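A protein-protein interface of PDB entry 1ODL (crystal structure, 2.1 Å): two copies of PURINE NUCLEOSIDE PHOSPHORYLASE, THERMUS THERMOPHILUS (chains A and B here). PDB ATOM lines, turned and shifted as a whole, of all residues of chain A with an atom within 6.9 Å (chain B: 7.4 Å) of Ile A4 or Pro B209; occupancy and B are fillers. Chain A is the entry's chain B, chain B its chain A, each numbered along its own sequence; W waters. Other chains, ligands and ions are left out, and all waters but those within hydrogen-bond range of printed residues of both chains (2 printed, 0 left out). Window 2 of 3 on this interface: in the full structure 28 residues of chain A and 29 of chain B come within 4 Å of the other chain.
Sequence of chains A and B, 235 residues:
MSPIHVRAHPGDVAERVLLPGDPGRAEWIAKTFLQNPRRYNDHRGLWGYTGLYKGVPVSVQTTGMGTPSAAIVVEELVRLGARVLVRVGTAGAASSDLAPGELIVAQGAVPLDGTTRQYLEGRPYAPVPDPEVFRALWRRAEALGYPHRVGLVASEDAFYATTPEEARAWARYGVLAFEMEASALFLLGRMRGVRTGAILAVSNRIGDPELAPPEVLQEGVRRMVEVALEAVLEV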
ATOM      1  N   SER A   2      21.291  17.505  21.962  1.00  0.00           N
ATOM      2  CA  SER A   2      21.839  17.116  20.629  1.00  0.00           C
ATOM      3  C   SER A   2      21.636  15.630  20.338  1.00  0.00           C
ATOM      4  O   SER A   2      21.693  14.795  21.245  1.00  0.00           O
ATOM      5  CB  SER A   2      23.334  17.444  20.562  1.00  0.00           C
ATOM      6  OG  SER A   2      23.906  16.971  19.356  1.00  0.00           O
ATOM      7  N   PRO A   3      21.393  15.281  19.061  1.00  0.00           N
ATOM      8  CA  PRO A   3      21.188  13.879  18.686  1.00  0.00           C
ATOM      9  C   PRO A   3      22.376  13.023  19.110  1.00  0.00           C
ATOM     10  O   PRO A   3      23.492  13.518  19.260  1.00  0.00           O
ATOM     11  CB  PRO A   3      21.026  13.948  17.171  1.00  0.00           C
ATOM     12  CG  PRO A   3      20.373  15.284  16.974  1.00  0.00           C
ATOM     13  CD  PRO A   3      21.180  16.167  17.901  1.00  0.00           C
ATOM     14  N   ILE A   4      22.125  11.737  19.303  1.00  0.00           N
ATOM     15  CA  ILE A   4      23.154  10.803  19.722  1.00  0.00           C
ATOM     16  C   ILE A   4      24.295  10.631  18.720  1.00  0.00           C
ATOM     17  O   ILE A   4      25.468  10.685  19.095  1.00  0.00           O
ATOM     18  CB  ILE A   4      22.538   9.418  19.993  1.00  0.00           C
ATOM     19  CG1 ILE A   4      21.496   9.524  21.115  1.00  0.00           C
ATOM     20  CG2 ILE A   4      23.628   8.429  20.343  1.00  0.00           C
ATOM     21  CD1 ILE A   4      20.597   8.300  21.243  1.00  0.00           C
ATOM     22  N   HIS A   5      23.953  10.439  17.450  1.00  0.00           N
ATOM     23  CA  HIS A   5      24.959  10.202  16.420  1.00  0.00           C
ATOM     24  C   HIS A   5      25.383  11.428  15.618  1.00  0.00           C
ATOM     25  O   HIS A   5      26.574  11.730  15.537  1.00  0.00           O
ATOM     26  CB  HIS A   5      24.470   9.086  15.508  1.00  0.00           C
ATOM     27  CG  HIS A   5      23.952   7.898  16.257  1.00  0.00           C
ATOM     28  ND1 HIS A   5      22.720   7.891  16.879  1.00  0.00           N
ATOM     29  CD2 HIS A   5      24.509   6.690  16.514  1.00  0.00           C
ATOM     30  CE1 HIS A   5      22.541   6.728  17.481  1.00  0.00           C
ATOM     31  NE2 HIS A   5      23.611   5.982  17.275  1.00  0.00           N
ATOM     32  N   VAL A   6      24.432  12.122  15.008  1.00  0.00           N
ATOM     33  CA  VAL A   6      24.781  13.336  14.280  1.00  0.00           C
ATOM     34  C   VAL A   6      24.721  14.423  15.349  1.00  0.00           C
ATOM     35  O   VAL A   6      23.655  14.976  15.636  1.00  0.00           O
ATOM     36  CB  VAL A   6      23.778  13.657  13.151  1.00  0.00           C
ATOM     37  CG1 VAL A   6      24.156  14.984  12.494  1.00  0.00           C
ATOM     38  CG2 VAL A   6      23.785  12.530  12.107  1.00  0.00           C
ATOM     39  N   ARG A   7      25.872  14.709  15.949  1.00  0.00           N
ATOM     40  CA  ARG A   7      25.959  15.699  17.022  1.00  0.00           C
ATOM     41  C   ARG A   7      25.988  17.152  16.569  1.00  0.00           C
ATOM     42  O   ARG A   7      27.000  17.840  16.693  1.00  0.00           O
ATOM     43  CB  ARG A   7      27.169  15.379  17.904  1.00  0.00           C
ATOM     44  CG  ARG A   7      26.986  14.067  18.661  1.00  0.00           C
ATOM     45  CD  ARG A   7      28.171  13.711  19.536  1.00  0.00           C
ATOM     46  NE  ARG A   7      27.900  12.494  20.298  1.00  0.00           N
ATOM     47  CZ  ARG A   7      28.787  11.872  21.069  1.00  0.00           C
ATOM     48  NH1 ARG A   7      30.020  12.348  21.188  1.00  0.00           N
ATOM     49  NH2 ARG A   7      28.437  10.771  21.726  1.00  0.00           N
ATOM     50  N   HIS A  43      31.393  13.413  14.185  1.00  0.00           N
ATOM     51  CA  HIS A  43      31.279  12.309  15.132  1.00  0.00           C
ATOM     52  C   HIS A  43      30.901  11.030  14.383  1.00  0.00           C
ATOM     53  O   HIS A  43      30.060  11.060  13.480  1.00  0.00           O
ATOM     54  CB  HIS A  43      30.218  12.610  16.190  1.00  0.00           C
ATOM     55  CG  HIS A  43      30.125  11.562  17.253  1.00  0.00           C
ATOM     56  ND1 HIS A  43      28.960  10.877  17.528  1.00  0.00           N
ATOM     57  CD2 HIS A  43      31.064  11.051  18.083  1.00  0.00           C
ATOM     58  CE1 HIS A  43      29.188   9.986  18.477  1.00  0.00           C
ATOM     59  NE2 HIS A  43      30.457  10.072  18.830  1.00  0.00           N
ATOM     60  N   ARG A  44      31.523   9.915  14.763  1.00  0.00           N
ATOM     61  CA  ARG A  44      31.280   8.621  14.119  1.00  0.00           C
ATOM     62  C   ARG A  44      31.544   8.678  12.615  1.00  0.00           C
ATOM     63  O   ARG A  44      31.009   7.881  11.848  1.00  0.00           O
ATOM     64  CB  ARG A  44      29.846   8.141  14.374  1.00  0.00           C
ATOM     65  CG  ARG A  44      29.663   7.379  15.694  1.00  0.00           C
ATOM     66  CD  ARG A  44      28.217   6.922  15.887  1.00  0.00           C
ATOM     67  NE  ARG A  44      28.020   6.139  17.112  1.00  0.00           N
ATOM     68  CZ  ARG A  44      28.394   4.870  17.272  1.00  0.00           C
ATOM     69  NH1 ARG A  44      28.994   4.216  16.286  1.00  0.00           N
ATOM     70  NH2 ARG A  44      28.158   4.246  18.423  1.00  0.00           N
ATOM     71  N   ILE A  72      19.138   5.955  11.148  1.00  0.00           N
ATOM     72  CA  ILE A  72      19.592   6.695  12.313  1.00  0.00           C
ATOM     73  C   ILE A  72      19.853   8.151  11.936  1.00  0.00           C
ATOM     74  O   ILE A  72      19.432   9.066  12.645  1.00  0.00           O
ATOM     75  CB  ILE A  72      20.879   6.058  12.879  1.00  0.00           C
ATOM     76  CG1 ILE A  72      20.515   4.788  13.658  1.00  0.00           C
ATOM     77  CG2 ILE A  72      21.647   7.063  13.725  1.00  0.00           C
ATOM     78  CD1 ILE A  72      21.720   4.011  14.177  1.00  0.00           C
ATOM     79  N   GLU A  76      17.492  11.540  12.922  1.00  0.00           N
ATOM     80  CA  GLU A  76      18.100  12.653  13.638  1.00  0.00           C
ATOM     81  C   GLU A  76      18.086  13.920  12.785  1.00  0.00           C
ATOM     82  O   GLU A  76      17.973  15.024  13.316  1.00  0.00           O
ATOM     83  CB  GLU A  76      19.525  12.278  14.075  1.00  0.00           C
ATOM     84  CG  GLU A  76      19.547  10.976  14.894  1.00  0.00           C
ATOM     85  CD  GLU A  76      20.893  10.650  15.513  1.00  0.00           C
ATOM     86  OE1 GLU A  76      21.926  11.175  15.050  1.00  0.00           O
ATOM     87  OE2 GLU A  76      20.915   9.845  16.465  1.00  0.00           O
ATOM     88  N   PHE B 159      17.191   1.269  14.985  1.00  0.00           N
ATOM     89  CA  PHE B 159      17.573   1.840  16.271  1.00  0.00           C
ATOM     90  C   PHE B 159      16.423   2.601  16.920  1.00  0.00           C
ATOM     91  O   PHE B 159      16.143   2.416  18.103  1.00  0.00           O
ATOM     92  CB  PHE B 159      18.764   2.786  16.092  1.00  0.00           C
ATOM     93  CG  PHE B 159      19.270   3.395  17.383  1.00  0.00           C
ATOM     94  CD1 PHE B 159      20.194   2.719  18.181  1.00  0.00           C
ATOM     95  CD2 PHE B 159      18.829   4.653  17.793  1.00  0.00           C
ATOM     96  CE1 PHE B 159      20.677   3.290  19.368  1.00  0.00           C
ATOM     97  CE2 PHE B 159      19.302   5.233  18.976  1.00  0.00           C
ATOM     98  CZ  PHE B 159      20.230   4.550  19.765  1.00  0.00           C
ATOM     99  N   TYR B 160      15.756   3.453  16.144  1.00  0.00           N
ATOM    100  CA  TYR B 160      14.664   4.260  16.676  1.00  0.00           C
ATOM    101  C   TYR B 160      13.272   3.652  16.671  1.00  0.00           C
ATOM    102  O   TYR B 160      12.295   4.347  16.947  1.00  0.00           O
ATOM    103  CB  TYR B 160      14.629   5.611  15.965  1.00  0.00           C
ATOM    104  CG  TYR B 160      15.746   6.527  16.411  1.00  0.00           C
ATOM    105  CD1 TYR B 160      16.819   6.806  15.574  1.00  0.00           C
ATOM    106  CD2 TYR B 160      15.733   7.101  17.685  1.00  0.00           C
ATOM    107  CE1 TYR B 160      17.855   7.631  15.992  1.00  0.00           C
ATOM    108  CE2 TYR B 160      16.761   7.931  18.110  1.00  0.00           C
ATOM    109  CZ  TYR B 160      17.819   8.190  17.259  1.00  0.00           C
ATOM    110  OH  TYR B 160      18.850   8.995  17.671  1.00  0.00           O
ATOM    111  N   ASN B 204      24.075   3.008  27.902  1.00  0.00           N
ATOM    112  CA  ASN B 204      22.798   3.582  28.319  1.00  0.00           C
ATOM    113  C   ASN B 204      21.722   2.520  28.501  1.00  0.00           C
ATOM    114  O   ASN B 204      21.819   1.418  27.961  1.00  0.00           O
ATOM    115  CB  ASN B 204      22.304   4.566  27.262  1.00  0.00           C
ATOM    116  CG  ASN B 204      22.101   3.900  25.912  1.00  0.00           C
ATOM    117  OD1 ASN B 204      23.060   3.466  25.274  1.00  0.00           O
ATOM    118  ND2 ASN B 204      20.849   3.804  25.477  1.00  0.00           N
ATOM    119  N   ARG B 205      20.693   2.860  29.269  1.00  0.00           N
ATOM    120  CA  ARG B 205      19.574   1.953  29.472  1.00  0.00           C
ATOM    121  C   ARG B 205      18.589   2.394  28.396  1.00  0.00           C
ATOM    122  O   ARG B 205      18.084   3.510  28.445  1.00  0.00           O
ATOM    123  CB  ARG B 205      18.957   2.139  30.866  1.00  0.00           C
ATOM    124  CG  ARG B 205      19.936   2.022  32.034  1.00  0.00           C
ATOM    125  CD  ARG B 205      19.198   2.161  33.367  1.00  0.00           C
ATOM    126  NE  ARG B 205      20.056   2.639  34.451  1.00  0.00           N
ATOM    127  CZ  ARG B 205      21.012   1.924  35.037  1.00  0.00           C
ATOM    128  NH1 ARG B 205      21.246   0.683  34.650  1.00  0.00           N
ATOM    129  NH2 ARG B 205      21.734   2.453  36.017  1.00  0.00           N
ATOM    130  N   ILE B 206      18.334   1.533  27.415  1.00  0.00           N
ATOM    131  CA  ILE B 206      17.423   1.869  26.321  1.00  0.00           C
ATOM    132  C   ILE B 206      16.279   2.812  26.677  1.00  0.00           C
ATOM    133  O   ILE B 206      15.560   2.603  27.659  1.00  0.00           O
ATOM    134  CB  ILE B 206      16.837   0.594  25.672  1.00  0.00           C
ATOM    135  CG1 ILE B 206      17.932  -0.111  24.868  1.00  0.00           C
ATOM    136  CG2 ILE B 206      15.651   0.946  24.775  1.00  0.00           C
ATOM    137  CD1 ILE B 206      17.444  -1.310  24.100  1.00  0.00           C
ATOM    138  N   GLY B 207      16.128   3.850  25.852  1.00  0.00           N
ATOM    139  CA  GLY B 207      15.086   4.841  26.043  1.00  0.00           C
ATOM    140  C   GLY B 207      15.646   6.207  26.399  1.00  0.00           C
ATOM    141  O   GLY B 207      14.934   7.216  26.352  1.00  0.00           O
ATOM    142  N   ASP B 208      16.925   6.243  26.762  1.00  0.00           N
ATOM    143  CA  ASP B 208      17.580   7.486  27.148  1.00  0.00           C
ATOM    144  C   ASP B 208      17.842   8.408  25.966  1.00  0.00           C
ATOM    145  O   ASP B 208      18.264   7.962  24.896  1.00  0.00           O
ATOM    146  CB  ASP B 208      18.904   7.193  27.855  1.00  0.00           C
ATOM    147  CG  ASP B 208      18.735   6.308  29.066  1.00  0.00           C
ATOM    148  OD1 ASP B 208      17.740   6.491  29.803  1.00  0.00           O
ATOM    149  OD2 ASP B 208      19.605   5.438  29.289  1.00  0.00           O
ATOM    150  N   PRO B 209      17.588   9.715  26.150  1.00  0.00           N
ATOM    151  CA  PRO B 209      17.795  10.723  25.106  1.00  0.00           C
ATOM    152  C   PRO B 209      19.274  10.882  24.757  1.00  0.00           C
ATOM    153  O   PRO B 209      19.618  11.247  23.633  1.00  0.00           O
ATOM    154  CB  PRO B 209      17.215  11.993  25.731  1.00  0.00           C
ATOM    155  CG  PRO B 209      16.148  11.463  26.645  1.00  0.00           C
ATOM    156  CD  PRO B 209      16.853  10.292  27.289  1.00  0.00           C
ATOM    157  N   GLU B 210      20.142  10.610  25.727  1.00  0.00           N
ATOM    158  CA  GLU B 210      21.582  10.729  25.522  1.00  0.00           C
ATOM    159  C   GLU B 210      22.327   9.549  26.143  1.00  0.00           C
ATOM    160  O   GLU B 210      21.740   8.735  26.860  1.00  0.00           O
ATOM    161  CB  GLU B 210      22.097  12.029  26.144  1.00  0.00           C
ATOM    162  CG  GLU B 210      21.212  13.235  25.890  1.00  0.00           C
ATOM    163  CD  GLU B 210      21.821  14.520  26.405  1.00  0.00           C
ATOM    164  OE1 GLU B 210      21.123  15.556  26.389  1.00  0.00           O
ATOM    165  OE2 GLU B 210      23.001  14.497  26.820  1.00  0.00           O
ATOM    166  N   LEU B 211      23.623   9.463  25.866  1.00  0.00           N
ATOM    167  CA  LEU B 211      24.452   8.390  26.401  1.00  0.00           C
ATOM    168  C   LEU B 211      24.942   8.775  27.794  1.00  0.00           C
ATOM    169  O   LEU B 211      24.761   9.915  28.230  1.00  0.00           O
ATOM    170  CB  LEU B 211      25.648   8.132  25.482  1.00  0.00           C
ATOM    171  CG  LEU B 211      25.327   7.791  24.023  1.00  0.00           C
ATOM    172  CD1 LEU B 211      26.622   7.578  23.253  1.00  0.00           C
ATOM    173  CD2 LEU B 211      24.449   6.547  23.961  1.00  0.00           C
HETATM  174  O   HOH W   1      21.982  12.934  23.174  1.00  0.00           O
HETATM  175  O   HOH W   2      19.224  10.802  19.574  1.00  0.00           O
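The guanidinium group (NE) of Arg A7 is in hydrogen-bond range of the backbone carbonyl oxygen (O) of Ile A4, 3.3 Å away.
A ring nitrogen (ND1) of His A43 lies within hydrogen-bond range of the backbone carbonyl oxygen (O) of His A5 (3.2 Å).
The side-chain carboxylate (OE2) of Glu A76 lies within hydrogen-bond range of a ring nitrogen (ND1) of His A5, at 2.7 Å.
OE1 of Glu A76 lies within hydrogen-bond range of N of Val A6, 2.7 Å away.
A ring nitrogen (NE2) of His A43 lies within hydrogen-bond range of the guanidinium group (NH1) of Arg A7 (3.3 Å).
Printed residues of chain A that touch a printed residue of chain B: Ile A4, His A5, Arg A7, Ile A72 and Glu A76.
Hydrophobic or aromatic side chains of chain A within 4 Å of the printed part of chain B: Ile A4, His A5 and Ile A72.
Of the 10 printed residues of chain B, 4 touch a printed residue of chain A.
Printed residues of chain B that touch a printed residue of chain A: Phe B159, Tyr B160, Pro B209 and Leu B211.
Among the printed residues, 6 pairs touch across the chains.
Among the printed residues, no Asp or Glu carboxylate lies within 4 Å of a Lys or Arg side-chain nitrogen of the other chain.
No position is printed for both chains.
Among the printed residues, pairs that only touch across the chains: Ile A4 with Pro B209, His A5 with Phe B159, Arg A7 with Leu B211, Ile A72 with Phe B159 and Ile A72 with Tyr B160.
The side-chain carboxylate (OE2) of Glu A76 lies within hydrogen-bond range of the side-chain hydroxyl (OH) of Tyr B160 (2.5 Å).
Ile A4 touches one residue of chain B.
Printed residues of chain B within 4 Å of Arg A7: Leu B211.
Pro B209 touches just one residue of chain A: Ile A4 (3.6 Å).
Of the printed residues of chain A, Leu B211 touches Arg A7.
The nearest printed residue of chain B that does not touch Ile A4 is Phe B159 (4.03 Å).
The nearest residue of chain A that does not touch Pro B209 is Ser A2 (4.8 Å).
Water W2 bridges OH of Tyr B160 (2.7 Å) and N of Ile A4 (3.1 Å).
Water W1 bridges O of Ser A2 and O of Pro B209.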
